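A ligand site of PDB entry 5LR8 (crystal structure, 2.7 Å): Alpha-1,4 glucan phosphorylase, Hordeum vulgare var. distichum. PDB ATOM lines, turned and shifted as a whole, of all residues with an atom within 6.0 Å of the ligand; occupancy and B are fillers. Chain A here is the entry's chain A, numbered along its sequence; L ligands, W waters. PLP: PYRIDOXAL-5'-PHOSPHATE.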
ATOM      1  N   LEU A  95     -15.576  -2.905  21.985  1.00  0.00           N
ATOM      2  CA  LEU A  95     -16.012  -4.303  22.115  1.00  0.00           C
ATOM      3  C   LEU A  95     -17.368  -4.357  22.812  1.00  0.00           C
ATOM      4  O   LEU A  95     -17.458  -4.695  23.986  1.00  0.00           O
ATOM      5  CB  LEU A  95     -14.979  -5.161  22.884  1.00  0.00           C
ATOM      6  CG  LEU A  95     -13.990  -6.034  22.108  1.00  0.00           C
ATOM      7  CD1 LEU A  95     -13.448  -7.123  23.024  1.00  0.00           C
ATOM      8  CD2 LEU A  95     -14.600  -6.677  20.870  1.00  0.00           C
ATOM      9  N   ASN A 138     -11.516  -4.998  19.384  1.00  0.00           N
ATOM     10  CA  ASN A 138     -10.537  -6.082  19.346  1.00  0.00           C
ATOM     11  C   ASN A 138     -10.207  -6.563  20.750  1.00  0.00           C
ATOM     12  O   ASN A 138     -10.579  -7.667  21.133  1.00  0.00           O
ATOM     13  CB  ASN A 138      -9.258  -5.614  18.620  1.00  0.00           C
ATOM     14  CG  ASN A 138      -8.174  -6.678  18.593  1.00  0.00           C
ATOM     15  OD1 ASN A 138      -6.989  -6.363  18.516  1.00  0.00           O
ATOM     16  ND2 ASN A 138      -8.586  -7.950  18.628  1.00  0.00           N
ATOM     17  N   GLY A 139      -9.519  -5.727  21.510  1.00  0.00           N
ATOM     18  CA  GLY A 139      -9.029  -6.098  22.823  1.00  0.00           C
ATOM     19  C   GLY A 139      -9.444  -5.128  23.897  1.00  0.00           C
ATOM     20  O   GLY A 139     -10.467  -4.454  23.787  1.00  0.00           O
ATOM     21  N   GLY A 140      -8.619  -5.047  24.932  1.00  0.00           N
ATOM     22  CA  GLY A 140      -8.928  -4.301  26.136  1.00  0.00           C
ATOM     23  C   GLY A 140      -9.266  -2.835  25.920  1.00  0.00           C
ATOM     24  O   GLY A 140     -10.159  -2.300  26.571  1.00  0.00           O
ATOM     25  N   ARG A 143     -12.868  -2.776  24.939  1.00  0.00           N
ATOM     26  CA  ARG A 143     -13.763  -3.296  25.960  1.00  0.00           C
ATOM     27  C   ARG A 143     -13.864  -2.326  27.119  1.00  0.00           C
ATOM     28  O   ARG A 143     -14.947  -2.137  27.671  1.00  0.00           O
ATOM     29  CB  ARG A 143     -13.284  -4.672  26.429  1.00  0.00           C
ATOM     30  CG  ARG A 143     -14.187  -5.380  27.430  1.00  0.00           C
ATOM     31  CD  ARG A 143     -15.652  -5.453  27.019  1.00  0.00           C
ATOM     32  NE  ARG A 143     -16.531  -4.704  27.925  1.00  0.00           N
ATOM     33  CZ  ARG A 143     -17.846  -4.592  27.792  1.00  0.00           C
ATOM     34  NH1 ARG A 143     -18.485  -5.155  26.771  1.00  0.00           N
ATOM     35  NH2 ARG A 143     -18.538  -3.901  28.689  1.00  0.00           N
ATOM     36  N   VAL A 573     -14.153  -2.652  35.358  1.00  0.00           N
ATOM     37  CA  VAL A 573     -15.088  -3.320  34.460  1.00  0.00           C
ATOM     38  C   VAL A 573     -16.492  -3.266  35.064  1.00  0.00           C
ATOM     39  O   VAL A 573     -16.633  -3.159  36.282  1.00  0.00           O
ATOM     40  CB  VAL A 573     -14.693  -4.783  34.230  1.00  0.00           C
ATOM     41  CG1 VAL A 573     -13.251  -4.860  33.734  1.00  0.00           C
ATOM     42  CG2 VAL A 573     -14.863  -5.610  35.509  1.00  0.00           C
ATOM     43  N   TRP A 578     -20.346  -8.442  33.750  1.00  0.00           N
ATOM     44  CA  TRP A 578     -19.267  -9.353  34.148  1.00  0.00           C
ATOM     45  C   TRP A 578     -19.475 -10.076  35.490  1.00  0.00           C
ATOM     46  O   TRP A 578     -18.607 -10.820  35.925  1.00  0.00           O
ATOM     47  CB  TRP A 578     -17.923  -8.625  34.085  1.00  0.00           C
ATOM     48  CG  TRP A 578     -17.564  -8.217  32.680  1.00  0.00           C
ATOM     49  CD1 TRP A 578     -17.434  -6.947  32.201  1.00  0.00           C
ATOM     50  CD2 TRP A 578     -17.328  -9.091  31.571  1.00  0.00           C
ATOM     51  NE1 TRP A 578     -17.115  -6.975  30.866  1.00  0.00           N
ATOM     52  CE2 TRP A 578     -17.036  -8.284  30.452  1.00  0.00           C
ATOM     53  CE3 TRP A 578     -17.316 -10.482  31.414  1.00  0.00           C
ATOM     54  CZ2 TRP A 578     -16.743  -8.809  29.195  1.00  0.00           C
ATOM     55  CZ3 TRP A 578     -17.019 -11.013  30.164  1.00  0.00           C
ATOM     56  CH2 TRP A 578     -16.745 -10.175  29.071  1.00  0.00           C
ATOM     57  N   VAL A 655      -6.240 -16.398  28.605  1.00  0.00           N
ATOM     58  CA  VAL A 655      -7.128 -15.829  27.620  1.00  0.00           C
ATOM     59  C   VAL A 655      -6.722 -14.366  27.373  1.00  0.00           C
ATOM     60  O   VAL A 655      -7.046 -13.462  28.141  1.00  0.00           O
ATOM     61  CB  VAL A 655      -8.602 -16.064  28.068  1.00  0.00           C
ATOM     62  CG1 VAL A 655      -9.382 -14.778  28.261  1.00  0.00           C
ATOM     63  CG2 VAL A 655      -9.308 -17.022  27.112  1.00  0.00           C
ATOM     64  N   LYS A 656      -5.940 -14.189  26.312  1.00  0.00           N
ATOM     65  CA  LYS A 656      -5.461 -12.873  25.878  1.00  0.00           C
ATOM     66  C   LYS A 656      -4.783 -12.995  24.524  1.00  0.00           C
ATOM     67  O   LYS A 656      -4.560 -14.100  24.043  1.00  0.00           O
ATOM     68  CB  LYS A 656      -4.545 -12.203  26.926  1.00  0.00           C
ATOM     69  CG  LYS A 656      -3.612 -13.127  27.712  1.00  0.00           C
ATOM     70  CD  LYS A 656      -3.060 -12.470  28.972  1.00  0.00           C
ATOM     71  CE  LYS A 656      -4.066 -12.388  30.135  1.00  0.00           C
ATOM     72  NZ  LYS A 656      -4.620 -11.019  30.351  1.00  0.00           N
ATOM     73  N   ARG A 657      -4.468 -11.846  23.914  1.00  0.00           N
ATOM     74  CA  ARG A 657      -3.930 -11.840  22.544  1.00  0.00           C
ATOM     75  C   ARG A 657      -2.574 -12.542  22.487  1.00  0.00           C
ATOM     76  O   ARG A 657      -1.724 -12.406  23.360  1.00  0.00           O
ATOM     77  CB  ARG A 657      -3.907 -10.425  21.937  1.00  0.00           C
ATOM     78  CG  ARG A 657      -2.545  -9.780  21.692  1.00  0.00           C
ATOM     79  CD  ARG A 657      -2.633  -8.856  20.475  1.00  0.00           C
ATOM     80  NE  ARG A 657      -3.176  -9.559  19.319  1.00  0.00           N
ATOM     81  CZ  ARG A 657      -3.779  -8.969  18.289  1.00  0.00           C
ATOM     82  NH1 ARG A 657      -4.236  -9.701  17.294  1.00  0.00           N
ATOM     83  NH2 ARG A 657      -3.929  -7.654  18.266  1.00  0.00           N
ATOM     84  N   LYS A 662       3.304 -11.644  26.210  1.00  0.00           N
ATOM     85  CA  LYS A 662       2.259 -12.149  27.099  1.00  0.00           C
ATOM     86  C   LYS A 662       2.607 -13.537  27.627  1.00  0.00           C
ATOM     87  O   LYS A 662       2.153 -13.943  28.699  1.00  0.00           O
ATOM     88  CB  LYS A 662       0.913 -12.159  26.381  1.00  0.00           C
ATOM     89  CG  LYS A 662       0.499 -10.786  25.866  1.00  0.00           C
ATOM     90  CD  LYS A 662      -0.866 -10.362  26.383  1.00  0.00           C
ATOM     91  CE  LYS A 662      -1.011  -8.863  26.409  1.00  0.00           C
ATOM     92  NZ  LYS A 662      -2.312  -8.444  26.986  1.00  0.00           N
ATOM     93  N   TYR A 740     -11.895 -16.267  20.231  1.00  0.00           N
ATOM     94  CA  TYR A 740     -12.147 -15.630  21.523  1.00  0.00           C
ATOM     95  C   TYR A 740     -12.713 -14.213  21.332  1.00  0.00           C
ATOM     96  O   TYR A 740     -12.154 -13.396  20.600  1.00  0.00           O
ATOM     97  CB  TYR A 740     -10.865 -15.588  22.359  1.00  0.00           C
ATOM     98  CG  TYR A 740     -11.028 -14.853  23.671  1.00  0.00           C
ATOM     99  CD1 TYR A 740     -11.683 -15.458  24.745  1.00  0.00           C
ATOM    100  CD2 TYR A 740     -10.524 -13.576  23.840  1.00  0.00           C
ATOM    101  CE1 TYR A 740     -11.825 -14.791  25.948  1.00  0.00           C
ATOM    102  CE2 TYR A 740     -10.667 -12.895  25.042  1.00  0.00           C
ATOM    103  CZ  TYR A 740     -11.322 -13.502  26.099  1.00  0.00           C
ATOM    104  OH  TYR A 740     -11.456 -12.835  27.296  1.00  0.00           O
ATOM    105  N   ASN A 741     -13.836 -13.948  21.998  1.00  0.00           N
ATOM    106  CA  ASN A 741     -14.504 -12.649  21.946  1.00  0.00           C
ATOM    107  C   ASN A 741     -15.367 -12.468  23.187  1.00  0.00           C
ATOM    108  O   ASN A 741     -15.369 -13.331  24.077  1.00  0.00           O
ATOM    109  CB  ASN A 741     -15.339 -12.537  20.657  1.00  0.00           C
ATOM    110  CG  ASN A 741     -16.429 -13.578  20.577  1.00  0.00           C
ATOM    111  OD1 ASN A 741     -16.732 -14.273  21.549  1.00  0.00           O
ATOM    112  ND2 ASN A 741     -17.040 -13.693  19.414  1.00  0.00           N
ATOM    113  N   VAL A 742     -16.106 -11.362  23.272  1.00  0.00           N
ATOM    114  CA  VAL A 742     -16.896 -11.076  24.474  1.00  0.00           C
ATOM    115  C   VAL A 742     -17.779 -12.273  24.843  1.00  0.00           C
ATOM    116  O   VAL A 742     -17.805 -12.687  26.009  1.00  0.00           O
ATOM    117  CB  VAL A 742     -17.770  -9.803  24.318  1.00  0.00           C
ATOM    118  CG1 VAL A 742     -18.611  -9.563  25.571  1.00  0.00           C
ATOM    119  CG2 VAL A 742     -16.896  -8.582  24.040  1.00  0.00           C
ATOM    120  N   SER A 743     -18.463 -12.841  23.863  1.00  0.00           N
ATOM    121  CA  SER A 743     -19.377 -13.959  24.112  1.00  0.00           C
ATOM    122  C   SER A 743     -18.668 -15.185  24.696  1.00  0.00           C
ATOM    123  O   SER A 743     -19.201 -15.840  25.598  1.00  0.00           O
ATOM    124  CB  SER A 743     -20.124 -14.334  22.837  1.00  0.00           C
ATOM    125  OG  SER A 743     -21.075 -13.351  22.532  1.00  0.00           O
ATOM    126  N   ALA A 745     -15.759 -15.127  26.411  1.00  0.00           N
ATOM    127  CA  ALA A 745     -15.387 -14.694  27.757  1.00  0.00           C
ATOM    128  C   ALA A 745     -16.528 -14.866  28.737  1.00  0.00           C
ATOM    129  O   ALA A 745     -16.335 -15.341  29.854  1.00  0.00           O
ATOM    130  CB  ALA A 745     -14.933 -13.248  27.739  1.00  0.00           C
ATOM    131  N   ILE A 749     -15.297 -17.156  31.634  1.00  0.00           N
ATOM    132  CA  ILE A 749     -14.832 -16.485  32.856  1.00  0.00           C
ATOM    133  C   ILE A 749     -15.508 -16.999  34.123  1.00  0.00           C
ATOM    134  O   ILE A 749     -14.806 -17.382  35.056  1.00  0.00           O
ATOM    135  CB  ILE A 749     -14.920 -14.945  32.716  1.00  0.00           C
ATOM    136  CG1 ILE A 749     -13.808 -14.442  31.781  1.00  0.00           C
ATOM    137  CG2 ILE A 749     -14.823 -14.271  34.090  1.00  0.00           C
ATOM    138  CD1 ILE A 749     -13.852 -12.964  31.445  1.00  0.00           C
ATOM    139  N   HIS A 757      -1.969 -14.518  34.193  1.00  0.00           N
ATOM    140  CA  HIS A 757      -1.634 -13.169  33.777  1.00  0.00           C
ATOM    141  C   HIS A 757      -0.134 -13.038  33.991  1.00  0.00           C
ATOM    142  O   HIS A 757       0.336 -12.411  34.939  1.00  0.00           O
ATOM    143  CB  HIS A 757      -2.441 -12.157  34.597  1.00  0.00           C
ATOM    144  CG  HIS A 757      -3.918 -12.404  34.547  1.00  0.00           C
ATOM    145  ND1 HIS A 757      -4.715 -11.972  33.509  1.00  0.00           N
ATOM    146  CD2 HIS A 757      -4.731 -13.099  35.379  1.00  0.00           C
ATOM    147  CE1 HIS A 757      -5.956 -12.360  33.721  1.00  0.00           C
ATOM    148  NE2 HIS A 757      -5.995 -13.050  34.847  1.00  0.00           N
ATOM    149  N   GLU A 764       2.990  -4.906  31.035  1.00  0.00           N
ATOM    150  CA  GLU A 764       1.558  -4.649  31.024  1.00  0.00           C
ATOM    151  C   GLU A 764       1.259  -3.361  31.774  1.00  0.00           C
ATOM    152  O   GLU A 764       1.849  -3.102  32.828  1.00  0.00           O
ATOM    153  CB  GLU A 764       0.806  -5.817  31.670  1.00  0.00           C
ATOM    154  CG  GLU A 764      -0.489  -6.188  30.957  1.00  0.00           C
ATOM    155  CD  GLU A 764      -0.248  -6.952  29.672  1.00  0.00           C
ATOM    156  OE1 GLU A 764      -0.799  -6.541  28.621  1.00  0.00           O
ATOM    157  OE2 GLU A 764       0.510  -7.944  29.714  1.00  0.00           O
ATOM    158  N   SER A 766      -2.200  -2.310  32.516  1.00  0.00           N
ATOM    159  CA  SER A 766      -3.250  -2.725  33.448  1.00  0.00           C
ATOM    160  C   SER A 766      -3.730  -4.154  33.180  1.00  0.00           C
ATOM    161  O   SER A 766      -3.120  -5.111  33.657  1.00  0.00           O
ATOM    162  CB  SER A 766      -4.428  -1.742  33.413  1.00  0.00           C
ATOM    163  OG  SER A 766      -5.569  -2.276  34.078  1.00  0.00           O
ATOM    164  N   GLY A 767      -4.814  -4.279  32.424  1.00  0.00           N
ATOM    165  CA  GLY A 767      -5.443  -5.565  32.144  1.00  0.00           C
ATOM    166  C   GLY A 767      -6.793  -5.578  32.831  1.00  0.00           C
ATOM    167  O   GLY A 767      -6.881  -5.343  34.030  1.00  0.00           O
ATOM    168  N   THR A 768      -7.851  -5.823  32.066  1.00  0.00           N
ATOM    169  CA  THR A 768      -9.204  -5.816  32.606  1.00  0.00           C
ATOM    170  C   THR A 768      -9.763  -7.228  32.788  1.00  0.00           C
ATOM    171  O   THR A 768     -10.600  -7.427  33.664  1.00  0.00           O
ATOM    172  CB  THR A 768     -10.171  -4.964  31.757  1.00  0.00           C
ATOM    173  OG1 THR A 768     -10.250  -5.463  30.417  1.00  0.00           O
ATOM    174  CG2 THR A 768      -9.701  -3.505  31.726  1.00  0.00           C
ATOM    175  N   SER A 769      -9.314  -8.187  31.992  1.00  0.00           N
ATOM    176  CA  SER A 769      -9.751  -9.580  32.173  1.00  0.00           C
ATOM    177  C   SER A 769      -9.395 -10.074  33.579  1.00  0.00           C
ATOM    178  O   SER A 769     -10.174 -10.775  34.215  1.00  0.00           O
ATOM    179  CB  SER A 769      -9.165 -10.517  31.080  1.00  0.00           C
ATOM    180  OG  SER A 769      -7.779 -10.779  31.254  1.00  0.00           O
ATOM    181  N   ASN A 770      -8.219  -9.657  34.048  1.00  0.00           N
ATOM    182  CA  ASN A 770      -7.770  -9.931  35.419  1.00  0.00           C
ATOM    183  C   ASN A 770      -8.853  -9.617  36.457  1.00  0.00           C
ATOM    184  O   ASN A 770      -9.124 -10.411  37.360  1.00  0.00           O
ATOM    185  CB  ASN A 770      -6.536  -9.084  35.755  1.00  0.00           C
ATOM    186  CG  ASN A 770      -5.498  -9.052  34.650  1.00  0.00           C
ATOM    187  OD1 ASN A 770      -5.807  -9.250  33.471  1.00  0.00           O
ATOM    188  ND2 ASN A 770      -4.257  -8.785  35.025  1.00  0.00           N
ATOM    189  N   LYS A 772     -12.099  -9.155  35.901  1.00  0.00           N
ATOM    190  CA  LYS A 772     -13.299  -9.957  35.631  1.00  0.00           C
ATOM    191  C   LYS A 772     -13.198 -11.308  36.325  1.00  0.00           C
ATOM    192  O   LYS A 772     -14.154 -11.767  36.956  1.00  0.00           O
ATOM    193  CB  LYS A 772     -13.481 -10.186  34.126  1.00  0.00           C
ATOM    194  CG  LYS A 772     -13.655  -8.917  33.294  1.00  0.00           C
ATOM    195  CD  LYS A 772     -13.591  -9.206  31.799  1.00  0.00           C
ATOM    196  CE  LYS A 772     -13.516  -7.918  30.992  1.00  0.00           C
ATOM    197  NZ  LYS A 772     -13.201  -8.148  29.557  1.00  0.00           N
HETATM  198  N1  PLP L   1     -11.109  -9.357  25.005  1.00  0.00           N
HETATM  199  C2  PLP L   1     -12.327  -9.649  25.492  1.00  0.00           C
HETATM  200  C2A PLP L   1     -13.325 -10.373  24.629  1.00  0.00           C
HETATM  201  C3  PLP L   1     -12.701  -9.278  26.870  1.00  0.00           C
HETATM  202  O3  PLP L   1     -13.928  -9.554  27.378  1.00  0.00           O
HETATM  203  C4  PLP L   1     -11.693  -8.574  27.677  1.00  0.00           C
HETATM  204  C4A PLP L   1     -12.035  -8.172  29.063  1.00  0.00           C
HETATM  205  C5  PLP L   1     -10.383  -8.310  27.026  1.00  0.00           C
HETATM  206  C6  PLP L   1     -10.167  -8.729  25.721  1.00  0.00           C
HETATM  207  C5A PLP L   1      -9.243  -7.613  27.725  1.00  0.00           C
HETATM  208  O4P PLP L   1      -8.371  -8.612  28.234  1.00  0.00           O
HETATM  209  P   PLP L   1      -6.933  -8.213  28.836  1.00  0.00           P
HETATM  210  O1P PLP L   1      -7.241  -7.141  29.831  1.00  0.00           O
HETATM  211  O2P PLP L   1      -6.454  -9.507  29.460  1.00  0.00           O
HETATM  212  O3P PLP L   1      -6.136  -7.765  27.642  1.00  0.00           O
HETATM  213  O   HOH W   1      -4.992  -8.908  25.254  1.00  0.00           O
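Leu 95 touches the ligand. CA of Gly 140 touches C5A of the ligand (3.7 Å). Arg 143 touches the ligand. Trp 578 touches the ligand. CE2 of Tyr 740 touches N1 of the ligand, 3.6 Å away. Asn 741 touches the ligand (C to C2A, 3.3 Å). Val 742 touches the ligand. CB of Ala 745 touches O3 of the ligand, at 3.8 Å. CA of Gly 767 touches O1P of the ligand, 3.3 Å away. Hydrophobic or aromatic side chains that line the ligand: Leu 95, Trp 578, Tyr 740 and Ala 745. Of the 25 residues printed, 14 come within 4 Å of the ligand. The nearest printed residue that does not touch the ligand is Asn 770 (4.1 Å).
OD1 of Asn 741 lies close to N of Ser 743 (3.2 Å). The backbone carbonyl oxygen (O) of Leu 95 lies within hydrogen-bond range of the guanidinium group (NH1) of Arg 143, 3.0 Å away. The side-chain amino group (NZ) of Lys 656 is in hydrogen-bond range of the side-chain hydroxyl (OG) of Ser 769, at 3.3 Å. The side-chain carboxylate (OE1) of Glu 764 is in salt-bridge range of the side-chain amino group (NZ) of Lys 662 (2.9 Å). ND1 of His 757 lies within hydrogen-bond range of NZ of Lys 656 (3.3 Å). The side-chain amide oxygen of Asn 770 is in hydrogen-bond range of the side-chain hydroxyl of Ser 769 (3.3 Å).
The side-chain amino group of Lys 772 is covalently linked to a carbon (C4A) of the ligand, 1.3 Å away. An oxygen (O2P) of the ligand sits at hydrogen-bond distance from the side-chain hydroxyl (OG) of Ser 769, at 2.6 Å. O3P of the ligand lies within salt-bridge range of NZ of Lys 662 (3.9 Å). An oxygen (O1P) of the ligand is in hydrogen-bond range of the backbone NH of Thr 768 (2.7 Å). The side-chain amino group (NZ) of Lys 656 lies within salt-bridge range of an oxygen (O2P) of the ligand, at 2.5 Å. OG1 of Thr 768 is in hydrogen-bond range of O1P of the ligand (3.5 Å). N of Ser 769 sits at hydrogen-bond distance from O1P of the ligand, 3.2 Å away.
Water W1 lies within hydrogen-bond range of an oxygen (O3P) of the ligand (2.9 Å), the side-chain amino group (NZ) of Lys 662 (3.2 Å) and the backbone NH (N) of Arg 657 (3.3 Å).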
